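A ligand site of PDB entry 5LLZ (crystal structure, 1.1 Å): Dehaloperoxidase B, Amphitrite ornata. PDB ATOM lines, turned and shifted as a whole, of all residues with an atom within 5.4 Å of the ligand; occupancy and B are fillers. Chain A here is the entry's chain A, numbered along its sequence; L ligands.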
ATOM      1  N   PHE A  21      23.180  -9.217   9.763  1.00  0.00           N
ATOM      2  CA  PHE A  21      21.831  -8.717   9.844  1.00  0.00           C
ATOM      3  C   PHE A  21      21.641  -7.754  11.064  1.00  0.00           C
ATOM      4  O   PHE A  21      20.929  -6.767  10.935  1.00  0.00           O
ATOM      5  CB  PHE A  21      20.774  -9.864   9.855  1.00  0.00           C
ATOM      6  CG  PHE A  21      19.494  -9.487   9.193  1.00  0.00           C
ATOM      7  CD1 PHE A  21      19.371  -9.590   7.788  1.00  0.00           C
ATOM      8  CD2 PHE A  21      18.485  -8.924   9.882  1.00  0.00           C
ATOM      9  CE1 PHE A  21      18.192  -9.252   7.143  1.00  0.00           C
ATOM     10  CE2 PHE A  21      17.296  -8.537   9.239  1.00  0.00           C
ATOM     11  CZ  PHE A  21      17.155  -8.695   7.860  1.00  0.00           C
ATOM     12  N   PHE A  24      23.008  -4.390  10.038  1.00  0.00           N
ATOM     13  CA  PHE A  24      21.974  -3.745   9.219  1.00  0.00           C
ATOM     14  C   PHE A  24      20.896  -3.062  10.120  1.00  0.00           C
ATOM     15  O   PHE A  24      20.620  -1.872   9.951  1.00  0.00           O
ATOM     16  CB  PHE A  24      21.350  -4.778   8.278  1.00  0.00           C
ATOM     17  CG  PHE A  24      20.039  -4.388   7.628  1.00  0.00           C
ATOM     18  CD1 PHE A  24      19.924  -3.298   6.743  1.00  0.00           C
ATOM     19  CD2 PHE A  24      18.886  -5.154   7.895  1.00  0.00           C
ATOM     20  CE1 PHE A  24      18.700  -2.998   6.167  1.00  0.00           C
ATOM     21  CE2 PHE A  24      17.659  -4.847   7.295  1.00  0.00           C
ATOM     22  CZ  PHE A  24      17.582  -3.753   6.435  1.00  0.00           C
ATOM     23  N   GLU A  31      14.392   0.538   9.886  1.00  0.00           N
ATOM     24  CA  GLU A  31      14.069  -0.702   9.172  1.00  0.00           C
ATOM     25  C   GLU A  31      13.306  -1.733   9.996  1.00  0.00           C
ATOM     26  O   GLU A  31      12.710  -2.661   9.428  1.00  0.00           O
ATOM     27  CB  GLU A  31      15.332  -1.364   8.576  1.00  0.00           C
ATOM     28  CG  GLU A  31      16.012  -0.561   7.476  1.00  0.00           C
ATOM     29  CD  GLU A  31      15.200  -0.590   6.176  1.00  0.00           C
ATOM     30  OE1 GLU A  31      14.877   0.472   5.591  1.00  0.00           O
ATOM     31  OE2 GLU A  31      14.830  -1.686   5.724  1.00  0.00           O
ATOM     32  N   ASN A  34       9.514  -2.970   9.277  1.00  0.00           N
ATOM     33  CA  ASN A  34       9.181  -4.292   8.614  1.00  0.00           C
ATOM     34  C   ASN A  34       9.285  -5.499   9.515  1.00  0.00           C
ATOM     35  O   ASN A  34       8.938  -6.607   9.077  1.00  0.00           O
ATOM     36  CB  ASN A  34      10.120  -4.632   7.411  1.00  0.00           C
ATOM     37  CG  ASN A  34      10.486  -3.418   6.590  1.00  0.00           C
ATOM     38  OD1 ASN A  34       9.672  -2.992   5.836  1.00  0.00           O
ATOM     39  ND2 ASN A  34      11.701  -2.827   6.805  1.00  0.00           N
ATOM     40  N   PHE A  35       9.837  -5.309  10.719  1.00  0.00           N
ATOM     41  CA  PHE A  35      10.117  -6.335  11.710  1.00  0.00           C
ATOM     42  C   PHE A  35       9.635  -5.831  13.094  1.00  0.00           C
ATOM     43  O   PHE A  35      10.438  -5.634  14.062  1.00  0.00           O
ATOM     44  CB  PHE A  35      11.628  -6.619  11.773  1.00  0.00           C
ATOM     45  CG  PHE A  35      12.212  -7.130  10.501  1.00  0.00           C
ATOM     46  CD1 PHE A  35      12.052  -8.460  10.110  1.00  0.00           C
ATOM     47  CD2 PHE A  35      12.957  -6.282   9.691  1.00  0.00           C
ATOM     48  CE1 PHE A  35      12.621  -8.934   8.928  1.00  0.00           C
ATOM     49  CE2 PHE A  35      13.521  -6.755   8.522  1.00  0.00           C
ATOM     50  CZ  PHE A  35      13.374  -8.081   8.136  1.00  0.00           C
ATOM     51  N   TYR A  38      10.922  -7.248  16.459  1.00  0.00           N
ATOM     52  CA  TYR A  38      12.295  -7.016  16.879  1.00  0.00           C
ATOM     53  C   TYR A  38      12.467  -5.703  17.709  1.00  0.00           C
ATOM     54  O   TYR A  38      13.561  -5.436  18.251  1.00  0.00           O
ATOM     55  CB  TYR A  38      13.191  -7.038  15.632  1.00  0.00           C
ATOM     56  CG  TYR A  38      13.245  -8.312  14.801  1.00  0.00           C
ATOM     57  CD1 TYR A  38      12.692  -9.528  15.221  1.00  0.00           C
ATOM     58  CD2 TYR A  38      13.909  -8.290  13.558  1.00  0.00           C
ATOM     59  CE1 TYR A  38      12.739 -10.665  14.414  1.00  0.00           C
ATOM     60  CE2 TYR A  38      13.933  -9.409  12.781  1.00  0.00           C
ATOM     61  CZ  TYR A  38      13.392 -10.590  13.195  1.00  0.00           C
ATOM     62  OH  TYR A  38      13.517 -11.667  12.343  1.00  0.00           O
ATOM     63  N   LYS A  51      12.341 -17.004  15.462  1.00  0.00           N
ATOM     64  CA  LYS A  51      12.090 -16.553  14.084  1.00  0.00           C
ATOM     65  C   LYS A  51      13.165 -15.606  13.597  1.00  0.00           C
ATOM     66  O   LYS A  51      13.407 -15.534  12.361  1.00  0.00           O
ATOM     67  CB  LYS A  51      10.751 -15.904  13.979  1.00  0.00           C
ATOM     68  CG  LYS A  51       9.606 -16.908  14.181  1.00  0.00           C
ATOM     69  CD  LYS A  51       8.315 -16.236  13.883  1.00  0.00           C
ATOM     70  CE  LYS A  51       7.145 -17.206  14.076  1.00  0.00           C
ATOM     71  NZ  LYS A  51       6.896 -18.061  12.879  1.00  0.00           N
ATOM     72  N   ASP A  54      15.647 -18.018  12.411  1.00  0.00           N
ATOM     73  CA  ASP A  54      15.112 -18.623  11.128  1.00  0.00           C
ATOM     74  C   ASP A  54      15.170 -17.783   9.911  1.00  0.00           C
ATOM     75  O   ASP A  54      15.759 -18.331   8.936  1.00  0.00           O
ATOM     76  CB  ASP A  54      13.639 -19.087  11.313  1.00  0.00           C
ATOM     77  CG  ASP A  54      13.506 -20.219  12.304  1.00  0.00           C
ATOM     78  OD1 ASP A  54      14.590 -20.717  12.742  1.00  0.00           O
ATOM     79  OD2 ASP A  54      12.347 -20.620  12.645  1.00  0.00           O
ATOM     80  N   HIS A  55      14.639 -16.538   9.893  1.00  0.00           N
ATOM     81  CA  HIS A  55      14.742 -15.570   8.744  1.00  0.00           C
ATOM     82  C   HIS A  55      16.156 -15.442   8.463  1.00  0.00           C
ATOM     83  O   HIS A  55      16.501 -15.663   7.326  1.00  0.00           O
ATOM     84  CB  HIS A  55      14.095 -14.145   8.945  1.00  0.00           C
ATOM     85  CG  HIS A  55      14.153 -13.235   7.696  1.00  0.00           C
ATOM     86  ND1 HIS A  55      14.739 -11.977   7.712  1.00  0.00           N
ATOM     87  CD2 HIS A  55      13.765 -13.427   6.407  1.00  0.00           C
ATOM     88  CE1 HIS A  55      14.682 -11.436   6.499  1.00  0.00           C
ATOM     89  NE2 HIS A  55      14.081 -12.289   5.691  1.00  0.00           N
ATOM     90  N   LYS A  58      17.873 -18.417   6.670  1.00  0.00           N
ATOM     91  CA  LYS A  58      17.388 -18.623   5.331  1.00  0.00           C
ATOM     92  C   LYS A  58      17.747 -17.459   4.377  1.00  0.00           C
ATOM     93  O   LYS A  58      18.077 -17.732   3.192  1.00  0.00           O
ATOM     94  CB  LYS A  58      15.886 -18.992   5.423  1.00  0.00           C
ATOM     95  CG  LYS A  58      15.768 -20.439   5.949  1.00  0.00           C
ATOM     96  CD  LYS A  58      14.424 -20.785   6.522  1.00  0.00           C
ATOM     97  CE  LYS A  58      14.240 -22.262   6.800  1.00  0.00           C
ATOM     98  NZ  LYS A  58      12.869 -22.422   7.404  1.00  0.00           N
ATOM     99  N   VAL A  59      17.817 -16.197   4.868  1.00  0.00           N
ATOM    100  CA  VAL A  59      18.311 -15.014   4.071  1.00  0.00           C
ATOM    101  C   VAL A  59      19.672 -15.397   3.532  1.00  0.00           C
ATOM    102  O   VAL A  59      19.935 -15.252   2.322  1.00  0.00           O
ATOM    103  CB  VAL A  59      18.459 -13.668   4.892  1.00  0.00           C
ATOM    104  CG1 VAL A  59      19.345 -12.616   4.185  1.00  0.00           C
ATOM    105  CG2 VAL A  59      17.138 -13.031   5.258  1.00  0.00           C
ATOM    106  N   LEU A  62      20.096 -18.548   1.053  1.00  0.00           N
ATOM    107  CA  LEU A  62      19.681 -18.199  -0.304  1.00  0.00           C
ATOM    108  C   LEU A  62      20.570 -17.148  -0.944  1.00  0.00           C
ATOM    109  O   LEU A  62      20.919 -17.239  -2.144  1.00  0.00           O
ATOM    110  CB  LEU A  62      18.206 -17.813  -0.404  1.00  0.00           C
ATOM    111  CG  LEU A  62      17.627 -17.551  -1.814  1.00  0.00           C
ATOM    112  CD1 LEU A  62      17.892 -18.681  -2.852  1.00  0.00           C
ATOM    113  CD2 LEU A  62      16.140 -17.208  -1.709  1.00  0.00           C
ATOM    114  N   MET A  63      20.982 -16.126  -0.168  1.00  0.00           N
ATOM    115  CA  MET A  63      21.882 -15.096  -0.737  1.00  0.00           C
ATOM    116  C   MET A  63      23.184 -15.714  -1.249  1.00  0.00           C
ATOM    117  O   MET A  63      23.649 -15.279  -2.320  1.00  0.00           O
ATOM    118  CB  MET A  63      22.238 -14.005   0.315  1.00  0.00           C
ATOM    119  CG  MET A  63      23.008 -12.824  -0.253  1.00  0.00           C
ATOM    120  SD  MET A  63      23.890 -11.810   1.001  1.00  0.00           S
ATOM    121  CE  MET A  63      22.513 -11.111   1.924  1.00  0.00           C
ATOM    122  N   LEU A  83      12.898 -13.531  -5.881  1.00  0.00           N
ATOM    123  CA  LEU A  83      12.951 -12.628  -4.735  1.00  0.00           C
ATOM    124  C   LEU A  83      11.815 -11.583  -4.696  1.00  0.00           C
ATOM    125  O   LEU A  83      11.248 -11.322  -3.617  1.00  0.00           O
ATOM    126  CB  LEU A  83      14.304 -11.914  -4.638  1.00  0.00           C
ATOM    127  CG  LEU A  83      15.473 -12.840  -4.310  1.00  0.00           C
ATOM    128  CD1 LEU A  83      16.811 -12.138  -4.527  1.00  0.00           C
ATOM    129  CD2 LEU A  83      15.462 -13.344  -2.874  1.00  0.00           C
ATOM    130  N   MET A  86       8.220 -13.475  -3.928  1.00  0.00           N
ATOM    131  CA  MET A  86       8.003 -14.109  -2.616  1.00  0.00           C
ATOM    132  C   MET A  86       6.918 -13.338  -1.831  1.00  0.00           C
ATOM    133  O   MET A  86       7.019 -12.115  -1.647  1.00  0.00           O
ATOM    134  CB  MET A  86       9.272 -14.092  -1.793  1.00  0.00           C
ATOM    135  CG  MET A  86      10.283 -15.103  -2.194  1.00  0.00           C
ATOM    136  SD  MET A  86      11.871 -14.845  -1.417  1.00  0.00           S
ATOM    137  CE  MET A  86      11.361 -14.777   0.267  1.00  0.00           C
ATOM    138  N   GLN A  88       6.273 -13.024   1.177  1.00  0.00           N
ATOM    139  CA  GLN A  88       6.882 -12.346   2.354  1.00  0.00           C
ATOM    140  C   GLN A  88       7.558 -11.010   2.093  1.00  0.00           C
ATOM    141  O   GLN A  88       7.773 -10.219   3.024  1.00  0.00           O
ATOM    142  CB  GLN A  88       7.936 -13.224   3.031  1.00  0.00           C
ATOM    143  CG  GLN A  88       7.405 -14.556   3.564  1.00  0.00           C
ATOM    144  CD  GLN A  88       7.591 -15.694   2.569  1.00  0.00           C
ATOM    145  OE1 GLN A  88       7.185 -15.571   1.398  1.00  0.00           O
ATOM    146  NE2 GLN A  88       8.205 -16.789   3.011  1.00  0.00           N
ATOM    147  N   HIS A  89       7.942 -10.791   0.835  1.00  0.00           N
ATOM    148  CA  HIS A  89       8.575  -9.564   0.394  1.00  0.00           C
ATOM    149  C   HIS A  89       7.573  -8.538  -0.235  1.00  0.00           C
ATOM    150  O   HIS A  89       8.024  -7.542  -0.818  1.00  0.00           O
ATOM    151  CB  HIS A  89       9.683  -9.936  -0.632  1.00  0.00           C
ATOM    152  CG  HIS A  89      10.899 -10.573  -0.026  1.00  0.00           C
ATOM    153  ND1 HIS A  89      11.901 -11.146  -0.790  1.00  0.00           N
ATOM    154  CD2 HIS A  89      11.270 -10.743   1.269  1.00  0.00           C
ATOM    155  CE1 HIS A  89      12.852 -11.599   0.006  1.00  0.00           C
ATOM    156  NE2 HIS A  89      12.506 -11.354   1.253  1.00  0.00           N
ATOM    157  N   LEU A  92       8.134  -4.708   0.464  1.00  0.00           N
ATOM    158  CA  LEU A  92       9.500  -4.212   0.291  1.00  0.00           C
ATOM    159  C   LEU A  92       9.717  -3.383  -0.983  1.00  0.00           C
ATOM    160  O   LEU A  92       9.005  -3.546  -1.985  1.00  0.00           O
ATOM    161  CB  LEU A  92      10.476  -5.390   0.349  1.00  0.00           C
ATOM    162  CG  LEU A  92      10.447  -6.257   1.606  1.00  0.00           C
ATOM    163  CD1 LEU A  92      11.608  -7.235   1.535  1.00  0.00           C
ATOM    164  CD2 LEU A  92      10.535  -5.441   2.897  1.00  0.00           C
ATOM    165  N   ASN A  96      15.306  -1.239   0.732  1.00  0.00           N
ATOM    166  CA  ASN A  96      15.515  -2.175   1.862  1.00  0.00           C
ATOM    167  C   ASN A  96      16.746  -3.044   1.551  1.00  0.00           C
ATOM    168  O   ASN A  96      17.600  -3.288   2.407  1.00  0.00           O
ATOM    169  CB  ASN A  96      14.261  -3.062   2.087  1.00  0.00           C
ATOM    170  CG  ASN A  96      13.000  -2.271   2.436  1.00  0.00           C
ATOM    171  OD1 ASN A  96      11.986  -2.324   1.711  1.00  0.00           O
ATOM    172  ND2 ASN A  96      13.009  -1.623   3.584  1.00  0.00           N
ATOM    173  N   PHE A  97      16.844  -3.495   0.280  1.00  0.00           N
ATOM    174  CA  PHE A  97      17.970  -4.308  -0.167  1.00  0.00           C
ATOM    175  C   PHE A  97      19.278  -3.486  -0.286  1.00  0.00           C
ATOM    176  O   PHE A  97      20.366  -3.978   0.102  1.00  0.00           O
ATOM    177  CB  PHE A  97      17.620  -5.011  -1.517  1.00  0.00           C
ATOM    178  CG  PHE A  97      16.586  -6.111  -1.346  1.00  0.00           C
ATOM    179  CD1 PHE A  97      15.222  -5.806  -1.271  1.00  0.00           C
ATOM    180  CD2 PHE A  97      16.957  -7.422  -1.205  1.00  0.00           C
ATOM    181  CE1 PHE A  97      14.284  -6.797  -1.053  1.00  0.00           C
ATOM    182  CE2 PHE A  97      16.037  -8.433  -1.025  1.00  0.00           C
ATOM    183  CZ  PHE A  97      14.678  -8.117  -0.955  1.00  0.00           C
ATOM    184  N   LEU A 100      20.711  -3.154   3.231  1.00  0.00           N
ATOM    185  CA  LEU A 100      21.302  -4.392   3.679  1.00  0.00           C
ATOM    186  C   LEU A 100      22.764  -4.530   3.170  1.00  0.00           C
ATOM    187  O   LEU A 100      23.707  -4.877   3.894  1.00  0.00           O
ATOM    188  CB  LEU A 100      20.434  -5.591   3.305  1.00  0.00           C
ATOM    189  CG  LEU A 100      21.030  -6.992   3.611  1.00  0.00           C
ATOM    190  CD1 LEU A 100      21.318  -7.184   5.118  1.00  0.00           C
ATOM    191  CD2 LEU A 100      20.136  -8.065   3.041  1.00  0.00           C
ATOM    192  N   PHE A 101      22.929  -4.280   1.854  1.00  0.00           N
ATOM    193  CA  PHE A 101      24.265  -4.425   1.250  1.00  0.00           C
ATOM    194  C   PHE A 101      25.253  -3.321   1.670  1.00  0.00           C
ATOM    195  O   PHE A 101      26.450  -3.627   1.833  1.00  0.00           O
ATOM    196  CB  PHE A 101      24.177  -4.641  -0.304  1.00  0.00           C
ATOM    197  CG  PHE A 101      23.740  -6.049  -0.633  1.00  0.00           C
ATOM    198  CD1 PHE A 101      24.681  -7.078  -0.657  1.00  0.00           C
ATOM    199  CD2 PHE A 101      22.431  -6.409  -0.794  1.00  0.00           C
ATOM    200  CE1 PHE A 101      24.330  -8.358  -0.847  1.00  0.00           C
ATOM    201  CE2 PHE A 101      22.055  -7.698  -0.992  1.00  0.00           C
ATOM    202  CZ  PHE A 101      22.982  -8.668  -1.013  1.00  0.00           C
ATOM    203  N   LEU A 127      22.224  -6.537  -7.836  1.00  0.00           N
ATOM    204  CA  LEU A 127      21.002  -7.183  -7.358  1.00  0.00           C
ATOM    205  C   LEU A 127      19.839  -6.190  -7.325  1.00  0.00           C
ATOM    206  O   LEU A 127      18.725  -6.485  -7.792  1.00  0.00           O
ATOM    207  CB  LEU A 127      21.216  -7.860  -6.013  1.00  0.00           C
ATOM    208  CG  LEU A 127      19.996  -8.647  -5.486  1.00  0.00           C
ATOM    209  CD1 LEU A 127      19.492  -9.711  -6.458  1.00  0.00           C
ATOM    210  CD2 LEU A 127      20.314  -9.215  -4.121  1.00  0.00           C
HETATM  211  C1  LIG L   1      11.476 -13.756   4.400  1.00  0.00           C
HETATM  212  C2  LIG L   1      15.433 -14.275   1.511  1.00  0.00           C
HETATM  213  C3  LIG L   1      16.184  -9.654   2.087  1.00  0.00           C
HETATM  214  C4  LIG L   1      12.268  -9.026   4.807  1.00  0.00           C
HETATM  215  C5  LIG L   1      12.480 -14.311   3.607  1.00  0.00           C
HETATM  216  C6  LIG L   1      12.779 -15.662   3.345  1.00  0.00           C
HETATM  217  C7  LIG L   1      13.918 -15.800   2.608  1.00  0.00           C
HETATM  218  C8  LIG L   1      14.294 -14.499   2.303  1.00  0.00           C
HETATM  219  C9  LIG L   1      14.539 -17.096   2.071  1.00  0.00           C
HETATM  220  C10 LIG L   1      12.012 -16.780   3.986  1.00  0.00           C
HETATM  221  C11 LIG L   1      12.574 -16.948   5.425  1.00  0.00           C
HETATM  222  C12 LIG L   1      11.707 -17.769   6.337  1.00  0.00           C
HETATM  223  O1  LIG L   1      12.206 -18.729   6.964  1.00  0.00           O
HETATM  224  O2  LIG L   1      10.498 -17.437   6.510  1.00  0.00           O
HETATM  225  C13 LIG L   1      16.071 -13.050   1.382  1.00  0.00           C
HETATM  226  C14 LIG L   1      17.234 -12.802   0.641  1.00  0.00           C
HETATM  227  C15 LIG L   1      17.475 -11.482   0.841  1.00  0.00           C
HETATM  228  C16 LIG L   1      16.324 -10.984   1.703  1.00  0.00           C
HETATM  229  C17 LIG L   1      18.054 -13.821  -0.112  1.00  0.00           C
HETATM  230  C18 LIG L   1      18.551 -10.652   0.248  1.00  0.00           C
HETATM  231  C19 LIG L   1      19.303 -11.013  -0.817  1.00  0.00           C
HETATM  232  C20 LIG L   1      15.185  -9.084   2.896  1.00  0.00           C
HETATM  233  C21 LIG L   1      15.198  -7.745   3.302  1.00  0.00           C
HETATM  234  C22 LIG L   1      14.061  -7.526   4.096  1.00  0.00           C
HETATM  235  C23 LIG L   1      13.412  -8.773   4.156  1.00  0.00           C
HETATM  236  C24 LIG L   1      16.224  -6.738   2.917  1.00  0.00           C
HETATM  237  C25 LIG L   1      13.628  -6.319   4.816  1.00  0.00           C
HETATM  238  C26 LIG L   1      14.401  -5.244   5.019  1.00  0.00           C
HETATM  239  C27 LIG L   1      11.825 -10.329   4.834  1.00  0.00           C
HETATM  240  C28 LIG L   1      10.632 -10.522   5.668  1.00  0.00           C
HETATM  241  C29 LIG L   1      10.407 -11.825   5.583  1.00  0.00           C
HETATM  242  C30 LIG L   1      11.487 -12.361   4.663  1.00  0.00           C
HETATM  243  C31 LIG L   1       9.774  -9.560   6.492  1.00  0.00           C
HETATM  244  C32 LIG L   1       9.210 -12.475   6.304  1.00  0.00           C
HETATM  245  C33 LIG L   1       9.130 -12.385   7.863  1.00  0.00           C
HETATM  246  C34 LIG L   1      10.446 -12.772   8.440  1.00  0.00           C
HETATM  247  O3  LIG L   1      10.855 -12.244   9.496  1.00  0.00           O
HETATM  248  O4  LIG L   1      11.111 -13.651   7.844  1.00  0.00           O
HETATM  249  N1  LIG L   1      13.399 -13.622   2.949  1.00  0.00           N
HETATM  250  N2  LIG L   1      15.491 -11.988   1.975  1.00  0.00           N
HETATM  251  N3  LIG L   1      14.106  -9.700   3.430  1.00  0.00           N
HETATM  252  N4  LIG L   1      12.326 -11.457   4.161  1.00  0.00           N
HETATM  253 FE1  LIG L   1      13.695 -11.692   3.170  1.00  0.00          FE
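Merely in contact with the ligand: Phe 97 (3.3 Å), Val 59 (3.4 Å), Met 86 (3.5 Å), Leu 92 (3.5 Å), Gln 88 (3.6 Å), Phe 35 (3.6 Å), Glu 31 (3.7 Å), Asn 96 (3.7 Å), Met 63 (3.7 Å), Phe 24 (3.8 Å), Leu 83 (3.8 Å), Leu 127 (3.9 Å) and Tyr 38 (3.9 Å).
The nearest printed residue that does not touch the ligand is Leu 62 (4.01 Å).
FE1 of the ligand is bound by NE2 of His 89 (2.3 Å).
A ring nitrogen (NE2) of His 55 sits close to a nitrogen (N4) of the ligand (2.5 Å).
The side-chain amino group (NZ) of Lys 58 is in salt-bridge range of an oxygen (O1) of the ligand, at 3.8 Å.
ND2 of Asn 34 sits at hydrogen-bond distance from O of Glu 31.
OE2 of Glu 31 lies within hydrogen-bond range of ND2 of Asn 96 (2.8 Å).
A ring nitrogen (ND1) of His 89 sits at hydrogen-bond distance from the backbone carbonyl oxygen of Leu 83, 2.9 Å away.
SD of Met 86 lies close to ND1 of His 89 (3.8 Å).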
